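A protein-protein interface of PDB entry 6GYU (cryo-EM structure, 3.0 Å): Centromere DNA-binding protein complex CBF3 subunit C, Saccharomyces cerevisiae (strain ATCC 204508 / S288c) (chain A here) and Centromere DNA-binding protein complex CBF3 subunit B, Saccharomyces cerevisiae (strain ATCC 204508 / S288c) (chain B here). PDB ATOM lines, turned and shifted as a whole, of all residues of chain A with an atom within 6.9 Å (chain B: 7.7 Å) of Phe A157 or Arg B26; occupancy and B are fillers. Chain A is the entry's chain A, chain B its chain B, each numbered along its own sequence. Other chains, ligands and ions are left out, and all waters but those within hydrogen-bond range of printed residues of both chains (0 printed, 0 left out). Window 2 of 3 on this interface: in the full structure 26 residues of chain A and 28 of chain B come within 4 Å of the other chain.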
ATOM      1  N   LYS A 149       7.730  15.678   8.392  1.00  0.00           N
ATOM      2  CA  LYS A 149       8.751  15.588   7.355  1.00  0.00           C
ATOM      3  C   LYS A 149       9.724  14.436   7.597  1.00  0.00           C
ATOM      4  O   LYS A 149       9.830  13.531   6.763  1.00  0.00           O
ATOM      5  CB  LYS A 149       9.504  16.916   7.237  1.00  0.00           C
ATOM      6  CG  LYS A 149      10.363  17.028   5.977  1.00  0.00           C
ATOM      7  CD  LYS A 149      11.844  16.784   6.229  1.00  0.00           C
ATOM      8  CE  LYS A 149      12.632  16.841   4.932  1.00  0.00           C
ATOM      9  NZ  LYS A 149      12.606  18.198   4.325  1.00  0.00           N
ATOM     10  N   ILE A 152       7.632  10.958  10.309  1.00  0.00           N
ATOM     11  CA  ILE A 152       6.435  10.327   9.752  1.00  0.00           C
ATOM     12  C   ILE A 152       6.659   9.919   8.301  1.00  0.00           C
ATOM     13  O   ILE A 152       6.434   8.763   7.929  1.00  0.00           O
ATOM     14  CB  ILE A 152       5.214  11.251   9.888  1.00  0.00           C
ATOM     15  CG1 ILE A 152       4.898  11.488  11.359  1.00  0.00           C
ATOM     16  CG2 ILE A 152       4.018  10.654   9.179  1.00  0.00           C
ATOM     17  CD1 ILE A 152       4.618  10.238  12.120  1.00  0.00           C
ATOM     18  N   ASP A 153       7.120  10.851   7.464  1.00  0.00           N
ATOM     19  CA  ASP A 153       7.375  10.513   6.068  1.00  0.00           C
ATOM     20  C   ASP A 153       8.625   9.664   5.892  1.00  0.00           C
ATOM     21  O   ASP A 153       8.818   9.092   4.814  1.00  0.00           O
ATOM     22  CB  ASP A 153       7.501  11.777   5.217  1.00  0.00           C
ATOM     23  CG  ASP A 153       6.182  12.495   5.036  1.00  0.00           C
ATOM     24  OD1 ASP A 153       5.132  11.829   5.100  1.00  0.00           O
ATOM     25  OD2 ASP A 153       6.194  13.725   4.825  1.00  0.00           O
ATOM     26  N   SER A 154       9.472   9.560   6.913  1.00  0.00           N
ATOM     27  CA  SER A 154      10.684   8.764   6.787  1.00  0.00           C
ATOM     28  C   SER A 154      10.428   7.271   6.933  1.00  0.00           C
ATOM     29  O   SER A 154      11.267   6.473   6.505  1.00  0.00           O
ATOM     30  CB  SER A 154      11.717   9.210   7.817  1.00  0.00           C
ATOM     31  OG  SER A 154      12.882   8.413   7.725  1.00  0.00           O
ATOM     32  N   VAL A 155       9.305   6.873   7.530  1.00  0.00           N
ATOM     33  CA  VAL A 155       8.928   5.471   7.589  1.00  0.00           C
ATOM     34  C   VAL A 155       7.682   5.169   6.766  1.00  0.00           C
ATOM     35  O   VAL A 155       7.483   4.014   6.370  1.00  0.00           O
ATOM     36  CB  VAL A 155       8.746   4.997   9.044  1.00  0.00           C
ATOM     37  CG1 VAL A 155      10.070   5.018   9.759  1.00  0.00           C
ATOM     38  CG2 VAL A 155       7.742   5.869   9.770  1.00  0.00           C
ATOM     39  N   ALA A 156       6.836   6.163   6.499  1.00  0.00           N
ATOM     40  CA  ALA A 156       5.743   6.004   5.545  1.00  0.00           C
ATOM     41  C   ALA A 156       6.311   6.268   4.156  1.00  0.00           C
ATOM     42  O   ALA A 156       6.204   7.362   3.598  1.00  0.00           O
ATOM     43  CB  ALA A 156       4.590   6.942   5.874  1.00  0.00           C
ATOM     44  N   PHE A 157       6.959   5.238   3.608  1.00  0.00           N
ATOM     45  CA  PHE A 157       7.539   5.336   2.274  1.00  0.00           C
ATOM     46  C   PHE A 157       6.448   5.459   1.217  1.00  0.00           C
ATOM     47  O   PHE A 157       6.386   6.448   0.478  1.00  0.00           O
ATOM     48  CB  PHE A 157       8.423   4.120   1.999  1.00  0.00           C
ATOM     49  CG  PHE A 157       9.665   4.069   2.836  1.00  0.00           C
ATOM     50  CD1 PHE A 157      10.791   4.788   2.471  1.00  0.00           C
ATOM     51  CD2 PHE A 157       9.709   3.300   3.988  1.00  0.00           C
ATOM     52  CE1 PHE A 157      11.939   4.742   3.239  1.00  0.00           C
ATOM     53  CE2 PHE A 157      10.855   3.249   4.762  1.00  0.00           C
ATOM     54  CZ  PHE A 157      11.971   3.971   4.386  1.00  0.00           C
ATOM     55  N   ASP A 158       5.575   4.459   1.136  1.00  0.00           N
ATOM     56  CA  ASP A 158       4.465   4.504   0.197  1.00  0.00           C
ATOM     57  C   ASP A 158       3.135   4.023   0.759  1.00  0.00           C
ATOM     58  O   ASP A 158       2.105   4.269   0.123  1.00  0.00           O
ATOM     59  CB  ASP A 158       4.807   3.693  -1.062  1.00  0.00           C
ATOM     60  CG  ASP A 158       5.237   2.266  -0.749  1.00  0.00           C
ATOM     61  OD1 ASP A 158       5.365   1.913   0.442  1.00  0.00           O
ATOM     62  OD2 ASP A 158       5.457   1.492  -1.704  1.00  0.00           O
ATOM     63  N   GLU A 159       3.108   3.360   1.913  1.00  0.00           N
ATOM     64  CA  GLU A 159       1.874   2.801   2.455  1.00  0.00           C
ATOM     65  C   GLU A 159       1.027   3.913   3.073  1.00  0.00           C
ATOM     66  O   GLU A 159       1.469   4.622   3.981  1.00  0.00           O
ATOM     67  CB  GLU A 159       2.195   1.679   3.443  1.00  0.00           C
ATOM     68  CG  GLU A 159       3.190   2.008   4.552  1.00  0.00           C
ATOM     69  CD  GLU A 159       3.475   0.821   5.444  1.00  0.00           C
ATOM     70  OE1 GLU A 159       2.889  -0.254   5.205  1.00  0.00           O
ATOM     71  OE2 GLU A 159       4.290   0.959   6.380  1.00  0.00           O
ATOM     72  N   LEU A 162      -0.234   4.713   7.054  1.00  0.00           N
ATOM     73  CA  LEU A 162       0.722   5.159   8.055  1.00  0.00           C
ATOM     74  C   LEU A 162       1.087   6.625   7.848  1.00  0.00           C
ATOM     75  O   LEU A 162       1.895   7.174   8.603  1.00  0.00           O
ATOM     76  CB  LEU A 162       1.947   4.234   8.011  1.00  0.00           C
ATOM     77  CG  LEU A 162       2.956   4.064   9.147  1.00  0.00           C
ATOM     78  CD1 LEU A 162       3.351   2.610   9.181  1.00  0.00           C
ATOM     79  CD2 LEU A 162       4.196   4.896   8.944  1.00  0.00           C
ATOM     80  N   LEU A 163       0.481   7.286   6.859  1.00  0.00           N
ATOM     81  CA  LEU A 163       0.614   8.732   6.737  1.00  0.00           C
ATOM     82  C   LEU A 163      -0.237   9.464   7.764  1.00  0.00           C
ATOM     83  O   LEU A 163       0.052  10.620   8.093  1.00  0.00           O
ATOM     84  CB  LEU A 163       0.209   9.203   5.337  1.00  0.00           C
ATOM     85  CG  LEU A 163       1.202   9.242   4.173  1.00  0.00           C
ATOM     86  CD1 LEU A 163       2.380  10.128   4.515  1.00  0.00           C
ATOM     87  CD2 LEU A 163       1.664   7.874   3.734  1.00  0.00           C
ATOM     88  N   THR B   5      14.267  -1.860  -4.782  1.00  0.00           N
ATOM     89  CA  THR B   5      14.129  -2.144  -3.348  1.00  0.00           C
ATOM     90  C   THR B   5      15.429  -2.619  -2.690  1.00  0.00           C
ATOM     91  O   THR B   5      15.560  -3.790  -2.318  1.00  0.00           O
ATOM     92  CB  THR B   5      12.998  -3.156  -3.125  1.00  0.00           C
ATOM     93  OG1 THR B   5      11.883  -2.786  -3.941  1.00  0.00           O
ATOM     94  CG2 THR B   5      12.505  -3.097  -1.678  1.00  0.00           C
ATOM     95  N   THR B   6      16.426  -1.746  -2.609  1.00  0.00           N
ATOM     96  CA  THR B   6      17.711  -2.132  -2.048  1.00  0.00           C
ATOM     97  C   THR B   6      17.744  -1.902  -0.538  1.00  0.00           C
ATOM     98  O   THR B   6      16.867  -1.263   0.044  1.00  0.00           O
ATOM     99  CB  THR B   6      18.847  -1.363  -2.720  1.00  0.00           C
ATOM    100  OG1 THR B   6      20.104  -1.911  -2.303  1.00  0.00           O
ATOM    101  CG2 THR B   6      18.796   0.106  -2.339  1.00  0.00           C
ATOM    102  N   GLN B   7      18.777  -2.450   0.096  1.00  0.00           N
ATOM    103  CA  GLN B   7      19.013  -2.254   1.519  1.00  0.00           C
ATOM    104  C   GLN B   7      19.486  -0.822   1.757  1.00  0.00           C
ATOM    105  O   GLN B   7      19.992  -0.165   0.840  1.00  0.00           O
ATOM    106  CB  GLN B   7      20.043  -3.281   2.013  1.00  0.00           C
ATOM    107  CG  GLN B   7      20.267  -3.385   3.522  1.00  0.00           C
ATOM    108  CD  GLN B   7      19.013  -3.776   4.272  1.00  0.00           C
ATOM    109  OE1 GLN B   7      18.374  -2.942   4.915  1.00  0.00           O
ATOM    110  NE2 GLN B   7      18.653  -5.050   4.197  1.00  0.00           N
ATOM    111  N   LEU B   8      19.291  -0.338   2.993  1.00  0.00           N
ATOM    112  CA  LEU B   8      19.682   0.999   3.454  1.00  0.00           C
ATOM    113  C   LEU B   8      18.984   2.090   2.633  1.00  0.00           C
ATOM    114  O   LEU B   8      19.590   2.791   1.826  1.00  0.00           O
ATOM    115  CB  LEU B   8      21.206   1.188   3.444  1.00  0.00           C
ATOM    116  CG  LEU B   8      22.046   0.368   4.424  1.00  0.00           C
ATOM    117  CD1 LEU B   8      23.527   0.579   4.158  1.00  0.00           C
ATOM    118  CD2 LEU B   8      21.706   0.731   5.859  1.00  0.00           C
ATOM    119  N   LYS B   9      17.669   2.158   2.824  1.00  0.00           N
ATOM    120  CA  LYS B   9      16.867   3.237   2.264  1.00  0.00           C
ATOM    121  C   LYS B   9      17.294   4.584   2.842  1.00  0.00           C
ATOM    122  O   LYS B   9      17.830   4.677   3.949  1.00  0.00           O
ATOM    123  CB  LYS B   9      15.380   3.019   2.561  1.00  0.00           C
ATOM    124  CG  LYS B   9      14.623   2.144   1.576  1.00  0.00           C
ATOM    125  CD  LYS B   9      14.868   0.664   1.780  1.00  0.00           C
ATOM    126  CE  LYS B   9      14.226   0.163   3.057  1.00  0.00           C
ATOM    127  NZ  LYS B   9      14.416  -1.303   3.224  1.00  0.00           N
ATOM    128  N   SER B  10      17.043   5.642   2.079  1.00  0.00           N
ATOM    129  CA  SER B  10      17.300   6.991   2.556  1.00  0.00           C
ATOM    130  C   SER B  10      16.074   7.532   3.282  1.00  0.00           C
ATOM    131  O   SER B  10      14.952   7.059   3.095  1.00  0.00           O
ATOM    132  CB  SER B  10      17.682   7.916   1.401  1.00  0.00           C
ATOM    133  OG  SER B  10      16.593   8.100   0.518  1.00  0.00           O
ATOM    134  N   LYS B  11      16.305   8.538   4.125  1.00  0.00           N
ATOM    135  CA  LYS B  11      15.223   9.105   4.924  1.00  0.00           C
ATOM    136  C   LYS B  11      14.407  10.102   4.114  1.00  0.00           C
ATOM    137  O   LYS B  11      13.194   9.947   3.950  1.00  0.00           O
ATOM    138  CB  LYS B  11      15.785   9.770   6.184  1.00  0.00           C
ATOM    139  CG  LYS B  11      16.175   8.801   7.288  1.00  0.00           C
ATOM    140  CD  LYS B  11      17.622   8.367   7.189  1.00  0.00           C
ATOM    141  CE  LYS B  11      18.013   7.525   8.383  1.00  0.00           C
ATOM    142  NZ  LYS B  11      17.276   6.234   8.400  1.00  0.00           N
ATOM    143  N   HIS B  12      15.060  11.137   3.614  1.00  0.00           N
ATOM    144  CA  HIS B  12      14.432  12.135   2.772  1.00  0.00           C
ATOM    145  C   HIS B  12      14.502  11.721   1.305  1.00  0.00           C
ATOM    146  O   HIS B  12      15.356  10.917   0.919  1.00  0.00           O
ATOM    147  CB  HIS B  12      15.123  13.479   2.979  1.00  0.00           C
ATOM    148  CG  HIS B  12      16.594  13.439   2.715  1.00  0.00           C
ATOM    149  ND1 HIS B  12      17.506  13.023   3.661  1.00  0.00           N
ATOM    150  CD2 HIS B  12      17.313  13.737   1.607  1.00  0.00           C
ATOM    151  CE1 HIS B  12      18.724  13.079   3.152  1.00  0.00           C
ATOM    152  NE2 HIS B  12      18.634  13.510   1.906  1.00  0.00           N
ATOM    153  N   PRO B  13      13.591  12.228   0.471  1.00  0.00           N
ATOM    154  CA  PRO B  13      13.773  12.097  -0.979  1.00  0.00           C
ATOM    155  C   PRO B  13      15.012  12.850  -1.435  1.00  0.00           C
ATOM    156  O   PRO B  13      15.390  13.869  -0.853  1.00  0.00           O
ATOM    157  CB  PRO B  13      12.496  12.718  -1.555  1.00  0.00           C
ATOM    158  CG  PRO B  13      11.494  12.572  -0.471  1.00  0.00           C
ATOM    159  CD  PRO B  13      12.255  12.750   0.807  1.00  0.00           C
ATOM    160  N   CYS B  14      15.644  12.333  -2.485  1.00  0.00           N
ATOM    161  CA  CYS B  14      16.945  12.830  -2.906  1.00  0.00           C
ATOM    162  C   CYS B  14      16.824  14.218  -3.528  1.00  0.00           C
ATOM    163  O   CYS B  14      15.737  14.695  -3.861  1.00  0.00           O
ATOM    164  CB  CYS B  14      17.595  11.874  -3.903  1.00  0.00           C
ATOM    165  SG  CYS B  14      16.792  11.830  -5.515  1.00  0.00           S
ATOM    166  N   CYS B  17      15.392  14.281  -7.349  1.00  0.00           N
ATOM    167  CA  CYS B  17      13.948  14.178  -7.526  1.00  0.00           C
ATOM    168  C   CYS B  17      13.191  15.384  -6.986  1.00  0.00           C
ATOM    169  O   CYS B  17      12.047  15.604  -7.392  1.00  0.00           O
ATOM    170  CB  CYS B  17      13.427  12.898  -6.876  1.00  0.00           C
ATOM    171  SG  CYS B  17      13.938  11.390  -7.732  1.00  0.00           S
ATOM    172  N   LYS B  23       8.142  11.758  -8.305  1.00  0.00           N
ATOM    173  CA  LYS B  23       8.168  10.818  -7.194  1.00  0.00           C
ATOM    174  C   LYS B  23       9.586  10.308  -6.986  1.00  0.00           C
ATOM    175  O   LYS B  23      10.389  10.258  -7.921  1.00  0.00           O
ATOM    176  CB  LYS B  23       7.195   9.658  -7.448  1.00  0.00           C
ATOM    177  CG  LYS B  23       7.502   8.765  -8.660  1.00  0.00           C
ATOM    178  CD  LYS B  23       8.211   7.460  -8.284  1.00  0.00           C
ATOM    179  CE  LYS B  23       8.451   6.583  -9.499  1.00  0.00           C
ATOM    180  NZ  LYS B  23       9.187   5.339  -9.139  1.00  0.00           N
ATOM    181  N   CYS B  24       9.896   9.926  -5.753  1.00  0.00           N
ATOM    182  CA  CYS B  24      11.213   9.411  -5.410  1.00  0.00           C
ATOM    183  C   CYS B  24      11.083   7.948  -5.009  1.00  0.00           C
ATOM    184  O   CYS B  24      10.435   7.626  -4.009  1.00  0.00           O
ATOM    185  CB  CYS B  24      11.847  10.228  -4.288  1.00  0.00           C
ATOM    186  SG  CYS B  24      13.517   9.696  -3.849  1.00  0.00           S
ATOM    187  N   ASP B  25      11.703   7.066  -5.789  1.00  0.00           N
ATOM    188  CA  ASP B  25      11.894   5.688  -5.362  1.00  0.00           C
ATOM    189  C   ASP B  25      12.971   5.697  -4.292  1.00  0.00           C
ATOM    190  O   ASP B  25      14.156   5.532  -4.595  1.00  0.00           O
ATOM    191  CB  ASP B  25      12.287   4.798  -6.542  1.00  0.00           C
ATOM    192  CG  ASP B  25      12.434   3.342  -6.153  1.00  0.00           C
ATOM    193  OD1 ASP B  25      11.404   2.684  -5.901  1.00  0.00           O
ATOM    194  OD2 ASP B  25      13.581   2.852  -6.115  1.00  0.00           O
ATOM    195  N   ARG B  26      12.563   5.887  -3.037  1.00  0.00           N
ATOM    196  CA  ARG B  26      13.444   6.374  -1.983  1.00  0.00           C
ATOM    197  C   ARG B  26      14.425   5.295  -1.532  1.00  0.00           C
ATOM    198  O   ARG B  26      14.314   4.755  -0.428  1.00  0.00           O
ATOM    199  CB  ARG B  26      12.597   6.877  -0.812  1.00  0.00           C
ATOM    200  CG  ARG B  26      13.318   7.737   0.205  1.00  0.00           C
ATOM    201  CD  ARG B  26      12.376   8.124   1.317  1.00  0.00           C
ATOM    202  NE  ARG B  26      11.309   9.001   0.856  1.00  0.00           N
ATOM    203  CZ  ARG B  26      10.262   9.338   1.598  1.00  0.00           C
ATOM    204  NH1 ARG B  26       9.329  10.144   1.111  1.00  0.00           N
ATOM    205  NH2 ARG B  26      10.150   8.863   2.830  1.00  0.00           N
ATOM    206  N   MET B  27      15.374   4.960  -2.396  1.00  0.00           N
ATOM    207  CA  MET B  27      16.444   4.027  -2.094  1.00  0.00           C
ATOM    208  C   MET B  27      17.747   4.804  -1.954  1.00  0.00           C
ATOM    209  O   MET B  27      17.766   6.037  -1.954  1.00  0.00           O
ATOM    210  CB  MET B  27      16.573   2.964  -3.186  1.00  0.00           C
ATOM    211  CG  MET B  27      15.353   2.088  -3.429  1.00  0.00           C
ATOM    212  SD  MET B  27      14.711   1.199  -2.003  1.00  0.00           S
ATOM    213  CE  MET B  27      13.115   1.982  -1.809  1.00  0.00           C
ATOM    214  N   ILE B  28      18.845   4.070  -1.823  1.00  0.00           N
ATOM    215  CA  ILE B  28      20.186   4.607  -2.009  1.00  0.00           C
ATOM    216  C   ILE B  28      20.848   3.809  -3.125  1.00  0.00           C
ATOM    217  O   ILE B  28      21.091   2.614  -2.954  1.00  0.00           O
ATOM    218  CB  ILE B  28      21.035   4.573  -0.724  1.00  0.00           C
ATOM    219  CG1 ILE B  28      20.498   5.602   0.274  1.00  0.00           C
ATOM    220  CG2 ILE B  28      22.484   4.877  -1.019  1.00  0.00           C
ATOM    221  CD1 ILE B  28      21.223   5.616   1.604  1.00  0.00           C
ATOM    222  N   PRO B  29      21.132   4.417  -4.295  1.00  0.00           N
ATOM    223  CA  PRO B  29      20.875   5.839  -4.575  1.00  0.00           C
ATOM    224  C   PRO B  29      19.433   6.210  -4.957  1.00  0.00           C
ATOM    225  O   PRO B  29      18.934   7.158  -4.364  1.00  0.00           O
ATOM    226  CB  PRO B  29      21.815   6.126  -5.749  1.00  0.00           C
ATOM    227  CG  PRO B  29      21.984   4.815  -6.427  1.00  0.00           C
ATOM    228  CD  PRO B  29      21.929   3.776  -5.355  1.00  0.00           C
ATOM    229  N   CYS B  30      18.792   5.424  -5.826  1.00  0.00           N
ATOM    230  CA  CYS B  30      17.408   5.543  -6.291  1.00  0.00           C
ATOM    231  C   CYS B  30      17.103   4.421  -7.266  1.00  0.00           C
ATOM    232  O   CYS B  30      18.009   3.716  -7.716  1.00  0.00           O
ATOM    233  CB  CYS B  30      17.100   6.869  -7.004  1.00  0.00           C
ATOM    234  SG  CYS B  30      16.539   8.275  -6.026  1.00  0.00           S
ATOM    235  N   GLY B  31      15.828   4.256  -7.607  1.00  0.00           N
ATOM    236  CA  GLY B  31      15.492   3.563  -8.832  1.00  0.00           C
ATOM    237  C   GLY B  31      15.299   4.526  -9.980  1.00  0.00           C
ATOM    238  O   GLY B  31      15.409   4.136 -11.146  1.00  0.00           O
ATOM    239  N   ASN B  32      15.044   5.795  -9.670  1.00  0.00           N
ATOM    240  CA  ASN B  32      14.706   6.804 -10.663  1.00  0.00           C
ATOM    241  C   ASN B  32      15.943   7.562 -11.135  1.00  0.00           C
ATOM    242  O   ASN B  32      15.954   8.109 -12.243  1.00  0.00           O
ATOM    243  CB  ASN B  32      13.672   7.766 -10.070  1.00  0.00           C
ATOM    244  CG  ASN B  32      12.894   8.528 -11.122  1.00  0.00           C
ATOM    245  OD1 ASN B  32      13.097   8.354 -12.323  1.00  0.00           O
ATOM    246  ND2 ASN B  32      11.980   9.376 -10.670  1.00  0.00           N
ATOM    247  N   LYS B 364       0.636  -4.072   4.541  1.00  0.00           N
ATOM    248  CA  LYS B 364       1.471  -4.765   5.506  1.00  0.00           C
ATOM    249  C   LYS B 364       0.737  -4.890   6.838  1.00  0.00           C
ATOM    250  O   LYS B 364      -0.014  -3.989   7.222  1.00  0.00           O
ATOM    251  CB  LYS B 364       2.786  -4.017   5.710  1.00  0.00           C
ATOM    252  CG  LYS B 364       3.685  -4.001   4.495  1.00  0.00           C
ATOM    253  CD  LYS B 364       4.991  -3.288   4.783  1.00  0.00           C
ATOM    254  CE  LYS B 364       5.953  -3.430   3.614  1.00  0.00           C
ATOM    255  NZ  LYS B 364       5.455  -2.742   2.393  1.00  0.00           N
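The guanidinium group (NH2) of Arg B26 sits at hydrogen-bond distance from the backbone carbonyl oxygen (O) of Asp A153 (2.4 Å).
The side-chain hydroxyl (OG) of Ser B10 is in hydrogen-bond range of the backbone carbonyl oxygen (O) of Met B27 (3.4 Å). The backbone carbonyl oxygen (O) of Lys B11 lies close to the guanidinium group (NH2) of Arg B26 (3.4 Å). The side-chain hydroxyl of Ser B10 is in hydrogen-bond range of the backbone carbonyl oxygen of His B12, at 3.1 Å.
Lys B11 touches Ser A154. Ser A154 touches Arg B26. Lys B9 touches Phe A157. Phe A157 touches Ser B10 (CE1 to O, 3.8 Å). Arg B26 touches Phe A157. Lys B364 touches Glu A159 (CD to OE1, 3.7 Å).
Of the printed residues of chain B, Asp A153 touches Arg B26. Of the printed residues of chain B, Ser A154 touches Lys B11 (3.3 Å) and Arg B26 (3.99 Å). Of chain B, only Lys B9, Ser B10 and Arg B26 come within 4 Å of Phe A157. Printed residues of chain B within 4 Å of Glu A159: Lys B364. Leu A163 touches none of the printed residues of chain B. Printed residues of chain A within 4 Å of Ser B10: Phe A157. Cys B24 touches none of the printed residues of chain A. Printed residues of chain A within 4 Å of Arg B26: Asp A153 (2.4 Å), Ser A154 (3.99 Å) and Phe A157 (3.9 Å). Printed residues of chain A within 4 Å of Lys B364: Glu A159. The nearest residue of chain B that does not touch Phe A157 is Lys B11 (5.4 Å).
Printed residues of chain A that touch a printed residue of chain B: Asp A153, Ser A154, Phe A157 and Glu A159. Hydrophobic or aromatic side chains of chain A that line the printed part of chain B: Phe A157. Of the 22 printed residues of chain B, 5 touch a printed residue of chain A. Along chain B the printed residues that touch a printed residue of chain A span positions 9 to 364. Among the printed residues, 7 pairs touch across the chains.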
